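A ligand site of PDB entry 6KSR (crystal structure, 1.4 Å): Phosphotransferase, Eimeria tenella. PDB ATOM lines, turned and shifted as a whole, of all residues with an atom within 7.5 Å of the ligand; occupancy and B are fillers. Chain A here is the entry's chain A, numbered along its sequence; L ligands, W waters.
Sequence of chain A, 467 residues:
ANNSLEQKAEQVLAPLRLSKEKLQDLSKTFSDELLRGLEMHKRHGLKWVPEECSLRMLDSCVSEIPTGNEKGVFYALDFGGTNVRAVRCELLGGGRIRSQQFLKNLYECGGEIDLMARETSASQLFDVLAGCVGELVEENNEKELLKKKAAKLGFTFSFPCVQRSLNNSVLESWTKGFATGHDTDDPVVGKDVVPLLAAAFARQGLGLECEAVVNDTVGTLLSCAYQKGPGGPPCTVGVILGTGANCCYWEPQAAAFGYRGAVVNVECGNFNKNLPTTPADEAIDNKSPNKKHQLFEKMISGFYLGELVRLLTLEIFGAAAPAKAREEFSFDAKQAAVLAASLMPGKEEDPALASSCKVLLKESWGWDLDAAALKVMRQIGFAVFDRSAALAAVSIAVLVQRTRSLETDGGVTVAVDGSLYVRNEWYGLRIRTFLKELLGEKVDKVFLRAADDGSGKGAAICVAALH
O4 of the ligand sits at hydrogen-bond distance from ND2 of Asn 246, 3.0 Å away.
The side-chain amide nitrogen (ND2) of Asn 215 is in hydrogen-bond range of an oxygen (O3) of the ligand.
OE2 of Glu 267 lies within hydrogen-bond range of O3 of the ligand, at 2.7 Å.
The side-chain carboxylate (OE1) of Glu 297 is in hydrogen-bond range of an oxygen (O1) of the ligand.
O1 of the ligand lies within hydrogen-bond range of O of Ala 245, 3.4 Å away.
The side-chain carboxylate of Asp 216 sits at hydrogen-bond distance from an oxygen (O4) of the ligand (2.5 Å).
ND2 of Asn 246 lies within hydrogen-bond range of OD1 of Asn 265 (2.9 Å).
N of Ala 245 lies within hydrogen-bond range of OE1 of Glu 297, 2.9 Å away.
The side-chain amide oxygen (OD1) of Asn 215 lies close to the side-chain carboxylate (OD1) of Asp 216.
The backbone NH of Gln 294 lies within hydrogen-bond range of the side-chain amide oxygen of Asn 270 (2.9 Å).
The backbone NH (N) of Ile 240 is in hydrogen-bond range of the backbone carbonyl oxygen (O) of Asn 246 (3.0 Å).
The side-chain hydroxyl of Thr 217 is in hydrogen-bond range of the side-chain amide oxygen of Asn 215, at 2.7 Å.
N of Glu 267 sits at hydrogen-bond distance from OD1 of Asn 246 (2.9 Å).
The side-chain amide nitrogen (NE2) of Gln 294 lies within hydrogen-bond range of the side-chain carboxylate (OE2) of Glu 297 (3.0 Å).
Merely in contact with the ligand: Thr 217 (3.5 Å), Gln 294 (3.6 Å), Ile 240 (3.7 Å) and Gly 244 (3.9 Å).
Hydrophobic or aromatic side chains that line the ligand: Ile 240.
Ten residues have an atom within 4 Å of the ligand: Asn 215, Asp 216, Thr 217, Ile 240, Gly 244, Ala 245, Asn 246, Glu 267, Gln 294 and Glu 297.
Along chain A the residues within 4 Å of the ligand span positions 215 to 297.
Water W2 lies within hydrogen-bond range of O1 of the ligand (2.9 Å), OE1 of Glu 267 (2.9 Å), N of Gly 269 (2.9 Å) and NE2 of Gln 294 (3.3 Å).
Water W6 lies within hydrogen-bond range of the backbone NH (N) of Gly 244, an oxygen (O6) of the ligand and the backbone NH (N) of Thr 243.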
ATOM      1  N   ARG A  56     -12.378  -5.379  17.177  1.00  0.00           N
ATOM      2  CA  ARG A  56     -12.062  -3.997  16.800  1.00  0.00           C
ATOM      3  C   ARG A  56     -12.811  -3.562  15.541  1.00  0.00           C
ATOM      4  O   ARG A  56     -13.068  -2.367  15.362  1.00  0.00           O
ATOM      5  CB  ARG A  56     -10.547  -3.796  16.634  1.00  0.00           C
ATOM      6  CG  ARG A  56      -9.785  -3.770  17.944  1.00  0.00           C
ATOM      7  CD  ARG A  56      -8.278  -3.775  17.662  1.00  0.00           C
ATOM      8  NE  ARG A  56      -7.453  -3.816  18.874  1.00  0.00           N
ATOM      9  CZ  ARG A  56      -6.909  -2.772  19.486  1.00  0.00           C
ATOM     10  NH1 ARG A  56      -7.102  -1.530  19.059  1.00  0.00           N
ATOM     11  NH2 ARG A  56      -6.164  -2.983  20.573  1.00  0.00           N
ATOM     12  N   LEU A  58     -11.994  -3.137  12.397  1.00  0.00           N
ATOM     13  CA  LEU A  58     -11.260  -2.024  11.797  1.00  0.00           C
ATOM     14  C   LEU A  58     -11.640  -1.798  10.342  1.00  0.00           C
ATOM     15  O   LEU A  58     -11.767  -2.742   9.550  1.00  0.00           O
ATOM     16  CB  LEU A  58      -9.759  -2.290  11.871  1.00  0.00           C
ATOM     17  CG  LEU A  58      -9.212  -2.436  13.290  1.00  0.00           C
ATOM     18  CD1 LEU A  58      -7.743  -2.838  13.263  1.00  0.00           C
ATOM     19  CD2 LEU A  58      -9.432  -1.166  14.107  1.00  0.00           C
ATOM     20  N   SER A 158       2.647  -4.526  10.280  1.00  0.00           N
ATOM     21  CA  SER A 158       1.903  -5.386  11.202  1.00  0.00           C
ATOM     22  C   SER A 158       2.106  -4.996  12.663  1.00  0.00           C
ATOM     23  O   SER A 158       2.661  -5.771  13.452  1.00  0.00           O
ATOM     24  CB  SER A 158       2.219  -6.861  10.956  1.00  0.00           C
ATOM     25  OG  SER A 158       1.967  -7.230   9.611  1.00  0.00           O
ATOM     26  N   PHE A 159       1.642  -3.809  13.015  1.00  0.00           N
ATOM     27  CA  PHE A 159       1.700  -3.257  14.358  1.00  0.00           C
ATOM     28  C   PHE A 159       0.393  -2.525  14.608  1.00  0.00           C
ATOM     29  O   PHE A 159      -0.319  -2.198  13.652  1.00  0.00           O
ATOM     30  CB  PHE A 159       2.885  -2.288  14.501  1.00  0.00           C
ATOM     31  CG  PHE A 159       4.226  -2.917  14.236  1.00  0.00           C
ATOM     32  CD1 PHE A 159       4.917  -3.554  15.254  1.00  0.00           C
ATOM     33  CD2 PHE A 159       4.803  -2.875  12.965  1.00  0.00           C
ATOM     34  CE1 PHE A 159       6.151  -4.131  15.024  1.00  0.00           C
ATOM     35  CE2 PHE A 159       6.039  -3.465  12.729  1.00  0.00           C
ATOM     36  CZ  PHE A 159       6.707  -4.087  13.761  1.00  0.00           C
ATOM     37  N   LYS A 176       6.360  -6.345  19.777  1.00  0.00           N
ATOM     38  CA  LYS A 176       7.313  -7.291  19.208  1.00  0.00           C
ATOM     39  C   LYS A 176       8.774  -6.906  19.472  1.00  0.00           C
ATOM     40  O   LYS A 176       9.656  -7.224  18.679  1.00  0.00           O
ATOM     41  CB  LYS A 176       7.070  -7.505  17.708  1.00  0.00           C
ATOM     42  CG  LYS A 176       5.686  -8.038  17.358  1.00  0.00           C
ATOM     43  CD  LYS A 176       5.336  -7.791  15.898  1.00  0.00           C
ATOM     44  CE  LYS A 176       3.977  -8.398  15.547  1.00  0.00           C
ATOM     45  NZ  LYS A 176       3.743  -8.474  14.070  1.00  0.00           N
ATOM     46  N   ASN A 215      -3.583  -4.774   6.280  1.00  0.00           N
ATOM     47  CA  ASN A 215      -3.442  -5.905   7.197  1.00  0.00           C
ATOM     48  C   ASN A 215      -3.262  -7.187   6.381  1.00  0.00           C
ATOM     49  O   ASN A 215      -3.800  -7.314   5.282  1.00  0.00           O
ATOM     50  CB  ASN A 215      -4.717  -6.044   8.051  1.00  0.00           C
ATOM     51  CG  ASN A 215      -4.693  -7.246   8.994  1.00  0.00           C
ATOM     52  OD1 ASN A 215      -5.334  -8.264   8.740  1.00  0.00           O
ATOM     53  ND2 ASN A 215      -3.954  -7.120  10.092  1.00  0.00           N
ATOM     54  N   ASP A 216      -2.538  -8.140   6.965  1.00  0.00           N
ATOM     55  CA  ASP A 216      -2.247  -9.384   6.263  1.00  0.00           C
ATOM     56  C   ASP A 216      -3.488 -10.175   5.864  1.00  0.00           C
ATOM     57  O   ASP A 216      -3.478 -10.836   4.817  1.00  0.00           O
ATOM     58  CB  ASP A 216      -1.180 -10.229   7.000  1.00  0.00           C
ATOM     59  CG  ASP A 216      -1.599 -10.647   8.418  1.00  0.00           C
ATOM     60  OD1 ASP A 216      -2.721 -10.308   8.879  1.00  0.00           O
ATOM     61  OD2 ASP A 216      -0.806 -11.367   9.070  1.00  0.00           O
ATOM     62  N   THR A 217      -4.580 -10.130   6.644  1.00  0.00           N
ATOM     63  CA  THR A 217      -5.785 -10.869   6.239  1.00  0.00           C
ATOM     64  C   THR A 217      -6.419 -10.247   5.006  1.00  0.00           C
ATOM     65  O   THR A 217      -6.930 -10.962   4.133  1.00  0.00           O
ATOM     66  CB  THR A 217      -6.839 -10.961   7.354  1.00  0.00           C
ATOM     67  OG1 THR A 217      -7.378  -9.653   7.642  1.00  0.00           O
ATOM     68  CG2 THR A 217      -6.273 -11.625   8.596  1.00  0.00           C
ATOM     69  N   VAL A 218      -6.382  -8.912   4.931  1.00  0.00           N
ATOM     70  CA  VAL A 218      -6.917  -8.204   3.772  1.00  0.00           C
ATOM     71  C   VAL A 218      -6.068  -8.487   2.544  1.00  0.00           C
ATOM     72  O   VAL A 218      -6.587  -8.758   1.458  1.00  0.00           O
ATOM     73  CB  VAL A 218      -7.010  -6.707   4.106  1.00  0.00           C
ATOM     74  CG1 VAL A 218      -7.467  -5.914   2.879  1.00  0.00           C
ATOM     75  CG2 VAL A 218      -7.980  -6.490   5.262  1.00  0.00           C
ATOM     76  N   VAL A 239      -8.798 -15.235   5.633  1.00  0.00           N
ATOM     77  CA  VAL A 239      -8.541 -15.939   6.893  1.00  0.00           C
ATOM     78  C   VAL A 239      -7.058 -16.254   7.006  1.00  0.00           C
ATOM     79  O   VAL A 239      -6.472 -16.784   6.061  1.00  0.00           O
ATOM     80  CB  VAL A 239      -9.329 -17.266   6.913  1.00  0.00           C
ATOM     81  CG1 VAL A 239      -9.002 -18.084   8.148  1.00  0.00           C
ATOM     82  CG2 VAL A 239     -10.830 -16.990   6.813  1.00  0.00           C
ATOM     83  N   ILE A 240      -6.477 -15.944   8.158  1.00  0.00           N
ATOM     84  CA  ILE A 240      -5.138 -16.427   8.493  1.00  0.00           C
ATOM     85  C   ILE A 240      -5.236 -17.323   9.716  1.00  0.00           C
ATOM     86  O   ILE A 240      -5.769 -16.925  10.759  1.00  0.00           O
ATOM     87  CB  ILE A 240      -4.132 -15.277   8.711  1.00  0.00           C
ATOM     88  CG1 ILE A 240      -3.857 -14.616   7.358  1.00  0.00           C
ATOM     89  CG2 ILE A 240      -2.814 -15.830   9.285  1.00  0.00           C
ATOM     90  CD1 ILE A 240      -2.994 -13.416   7.414  1.00  0.00           C
ATOM     91  N   LEU A 241      -4.723 -18.551   9.556  1.00  0.00           N
ATOM     92  CA  LEU A 241      -4.659 -19.570  10.606  1.00  0.00           C
ATOM     93  C   LEU A 241      -3.212 -20.037  10.666  1.00  0.00           C
ATOM     94  O   LEU A 241      -2.824 -21.017  10.023  1.00  0.00           O
ATOM     95  CB  LEU A 241      -5.643 -20.706  10.341  1.00  0.00           C
ATOM     96  CG  LEU A 241      -7.116 -20.280  10.402  1.00  0.00           C
ATOM     97  CD1 LEU A 241      -8.018 -21.284   9.687  1.00  0.00           C
ATOM     98  CD2 LEU A 241      -7.528 -20.118  11.848  1.00  0.00           C
ATOM     99  N   GLY A 242      -2.392 -19.288  11.395  1.00  0.00           N
ATOM    100  CA  GLY A 242      -0.960 -19.538  11.435  1.00  0.00           C
ATOM    101  C   GLY A 242      -0.449 -19.316  12.839  1.00  0.00           C
ATOM    102  O   GLY A 242      -1.041 -19.820  13.802  1.00  0.00           O
ATOM    103  N   THR A 243       0.641 -18.556  12.978  1.00  0.00           N
ATOM    104  CA  THR A 243       1.107 -18.214  14.311  1.00  0.00           C
ATOM    105  C   THR A 243       0.034 -17.463  15.082  1.00  0.00           C
ATOM    106  O   THR A 243      -0.170 -17.711  16.274  1.00  0.00           O
ATOM    107  CB  THR A 243       2.411 -17.406  14.215  1.00  0.00           C
ATOM    108  OG1 THR A 243       3.418 -18.211  13.588  1.00  0.00           O
ATOM    109  CG2 THR A 243       2.880 -17.010  15.603  1.00  0.00           C
ATOM    110  N   GLY A 244      -0.679 -16.558  14.400  1.00  0.00           N
ATOM    111  CA  GLY A 244      -1.857 -15.913  14.910  1.00  0.00           C
ATOM    112  C   GLY A 244      -3.088 -16.327  14.100  1.00  0.00           C
ATOM    113  O   GLY A 244      -2.985 -17.100  13.137  1.00  0.00           O
ATOM    114  N   ALA A 245      -4.249 -15.809  14.500  1.00  0.00           N
ATOM    115  CA  ALA A 245      -5.516 -16.151  13.852  1.00  0.00           C
ATOM    116  C   ALA A 245      -6.373 -14.909  13.726  1.00  0.00           C
ATOM    117  O   ALA A 245      -6.671 -14.255  14.737  1.00  0.00           O
ATOM    118  CB  ALA A 245      -6.274 -17.228  14.629  1.00  0.00           C
ATOM    119  N   ASN A 246      -6.796 -14.583  12.508  1.00  0.00           N
ATOM    120  CA  ASN A 246      -7.612 -13.388  12.286  1.00  0.00           C
ATOM    121  C   ASN A 246      -8.364 -13.568  10.992  1.00  0.00           C
ATOM    122  O   ASN A 246      -8.023 -14.421  10.157  1.00  0.00           O
ATOM    123  CB  ASN A 246      -6.737 -12.144  12.262  1.00  0.00           C
ATOM    124  CG  ASN A 246      -7.533 -10.826  12.188  1.00  0.00           C
ATOM    125  OD1 ASN A 246      -8.667 -10.726  12.642  1.00  0.00           O
ATOM    126  ND2 ASN A 246      -6.887  -9.797  11.634  1.00  0.00           N
ATOM    127  N   CYS A 247      -9.425 -12.785  10.817  1.00  0.00           N
ATOM    128  CA  CYS A 247     -10.162 -12.800   9.559  1.00  0.00           C
ATOM    129  C   CYS A 247     -10.602 -11.395   9.196  1.00  0.00           C
ATOM    130  O   CYS A 247     -10.726 -10.507  10.039  1.00  0.00           O
ATOM    131  CB  CYS A 247     -11.452 -13.631   9.622  1.00  0.00           C
ATOM    132  SG  CYS A 247     -11.320 -15.301  10.227  1.00  0.00           S
ATOM    133  N   ASN A 265     -11.471  -5.544   8.840  1.00  0.00           N
ATOM    134  CA  ASN A 265     -10.514  -6.383   9.553  1.00  0.00           C
ATOM    135  C   ASN A 265     -11.075  -6.621  10.954  1.00  0.00           C
ATOM    136  O   ASN A 265     -11.058  -5.717  11.793  1.00  0.00           O
ATOM    137  CB  ASN A 265      -9.149  -5.698   9.575  1.00  0.00           C
ATOM    138  CG  ASN A 265      -8.191  -6.373  10.547  1.00  0.00           C
ATOM    139  OD1 ASN A 265      -8.452  -7.484  11.010  1.00  0.00           O
ATOM    140  ND2 ASN A 265      -7.096  -5.706  10.862  1.00  0.00           N
ATOM    141  N   GLU A 267     -10.264  -8.469  13.573  1.00  0.00           N
ATOM    142  CA  GLU A 267      -9.413  -8.698  14.742  1.00  0.00           C
ATOM    143  C   GLU A 267     -10.090  -9.678  15.705  1.00  0.00           C
ATOM    144  O   GLU A 267     -10.170  -9.459  16.924  1.00  0.00           O
ATOM    145  CB  GLU A 267      -8.921  -7.401  15.402  1.00  0.00           C
ATOM    146  CG  GLU A 267      -7.904  -6.624  14.539  1.00  0.00           C
ATOM    147  CD  GLU A 267      -6.551  -7.349  14.355  1.00  0.00           C
ATOM    148  OE1 GLU A 267      -6.206  -8.262  15.144  1.00  0.00           O
ATOM    149  OE2 GLU A 267      -5.822  -6.957  13.417  1.00  0.00           O
ATOM    150  N   CYS A 268     -10.563 -10.779  15.133  1.00  0.00           N
ATOM    151  CA  CYS A 268     -11.350 -11.728  15.912  1.00  0.00           C
ATOM    152  C   CYS A 268     -10.516 -12.588  16.836  1.00  0.00           C
ATOM    153  O   CYS A 268     -11.102 -13.308  17.655  1.00  0.00           O
ATOM    154  CB  CYS A 268     -12.272 -12.577  15.018  1.00  0.00           C
ATOM    155  SG  CYS A 268     -11.498 -13.294  13.593  1.00  0.00           S
ATOM    156  N   GLY A 269      -9.191 -12.516  16.776  1.00  0.00           N
ATOM    157  CA  GLY A 269      -8.383 -13.222  17.767  1.00  0.00           C
ATOM    158  C   GLY A 269      -8.723 -12.790  19.181  1.00  0.00           C
ATOM    159  O   GLY A 269      -8.579 -13.577  20.129  1.00  0.00           O
ATOM    160  N   ASN A 270      -9.217 -11.557  19.352  1.00  0.00           N
ATOM    161  CA  ASN A 270      -9.586 -11.049  20.659  1.00  0.00           C
ATOM    162  C   ASN A 270     -11.018 -11.381  21.087  1.00  0.00           C
ATOM    163  O   ASN A 270     -11.413 -10.996  22.192  1.00  0.00           O
ATOM    164  CB  ASN A 270      -9.378  -9.526  20.690  1.00  0.00           C
ATOM    165  CG  ASN A 270      -9.336  -8.968  22.104  1.00  0.00           C
ATOM    166  OD1 ASN A 270      -8.517  -9.387  22.923  1.00  0.00           O
ATOM    167  ND2 ASN A 270     -10.239  -8.028  22.400  1.00  0.00           N
ATOM    168  N   GLN A 294      -6.647 -11.546  23.185  1.00  0.00           N
ATOM    169  CA  GLN A 294      -6.431 -12.596  22.187  1.00  0.00           C
ATOM    170  C   GLN A 294      -6.914 -13.973  22.654  1.00  0.00           C
ATOM    171  O   GLN A 294      -6.340 -14.995  22.271  1.00  0.00           O
ATOM    172  CB  GLN A 294      -4.969 -12.648  21.736  1.00  0.00           C
ATOM    173  CG  GLN A 294      -4.479 -11.335  21.101  1.00  0.00           C
ATOM    174  CD  GLN A 294      -5.336 -10.876  19.919  1.00  0.00           C
ATOM    175  OE1 GLN A 294      -6.107  -9.929  20.021  1.00  0.00           O
ATOM    176  NE2 GLN A 294      -5.170 -11.539  18.791  1.00  0.00           N
ATOM    177  N   GLU A 297      -7.852 -16.427  19.769  1.00  0.00           N
ATOM    178  CA  GLU A 297      -6.603 -16.840  19.156  1.00  0.00           C
ATOM    179  C   GLU A 297      -5.834 -17.853  20.024  1.00  0.00           C
ATOM    180  O   GLU A 297      -5.207 -18.770  19.488  1.00  0.00           O
ATOM    181  CB  GLU A 297      -5.763 -15.584  18.888  1.00  0.00           C
ATOM    182  CG  GLU A 297      -4.336 -15.826  18.419  1.00  0.00           C
ATOM    183  CD  GLU A 297      -3.682 -14.519  18.028  1.00  0.00           C
ATOM    184  OE1 GLU A 297      -3.745 -14.170  16.825  1.00  0.00           O
ATOM    185  OE2 GLU A 297      -3.172 -13.816  18.927  1.00  0.00           O
ATOM    186  N   SER A 301      -4.553 -20.713  17.455  1.00  0.00           N
ATOM    187  CA  SER A 301      -3.404 -20.489  16.589  1.00  0.00           C
ATOM    188  C   SER A 301      -2.201 -21.348  16.968  1.00  0.00           C
ATOM    189  O   SER A 301      -2.086 -21.895  18.068  1.00  0.00           O
ATOM    190  CB  SER A 301      -3.059 -18.997  16.548  1.00  0.00           C
ATOM    191  OG  SER A 301      -2.342 -18.632  17.714  1.00  0.00           O
HETATM  192  C1  LIG L   1      -2.920 -11.416  15.019  1.00  0.00           C
HETATM  193  C2  LIG L   1      -2.980  -9.954  14.617  1.00  0.00           C
HETATM  194  C3  LIG L   1      -3.890  -9.728  13.423  1.00  0.00           C
HETATM  195  C4  LIG L   1      -3.907 -10.883  12.432  1.00  0.00           C
HETATM  196  C5  LIG L   1      -3.210 -12.232  12.798  1.00  0.00           C
HETATM  197  C6  LIG L   1      -2.541 -13.040  11.677  1.00  0.00           C
HETATM  198  O1  LIG L   1      -4.234 -11.891  15.341  1.00  0.00           O
HETATM  199  O2  LIG L   1      -3.571  -9.212  15.696  1.00  0.00           O
HETATM  200  O3  LIG L   1      -3.636  -8.428  12.867  1.00  0.00           O
HETATM  201  O4  LIG L   1      -3.990 -10.518  11.049  1.00  0.00           O
HETATM  202  O5  LIG L   1      -2.368 -12.180  13.945  1.00  0.00           O
HETATM  203  O6  LIG L   1      -1.184 -12.649  11.412  1.00  0.00           O
HETATM  204  O   HOH W   1       0.466 -12.162  13.643  1.00  0.00           O
HETATM  205  O   HOH W   2      -6.850 -10.926  15.967  1.00  0.00           O
HETATM  206  O   HOH W   3      -1.064  -7.608  12.148  1.00  0.00           O
HETATM  207  O   HOH W   4      -2.758  -6.249  15.463  1.00  0.00           O
HETATM  208  O   HOH W   5      -2.417  -9.156  18.150  1.00  0.00           O
HETATM  209  O   HOH W   6       0.087 -15.391  11.795  1.00  0.00           O
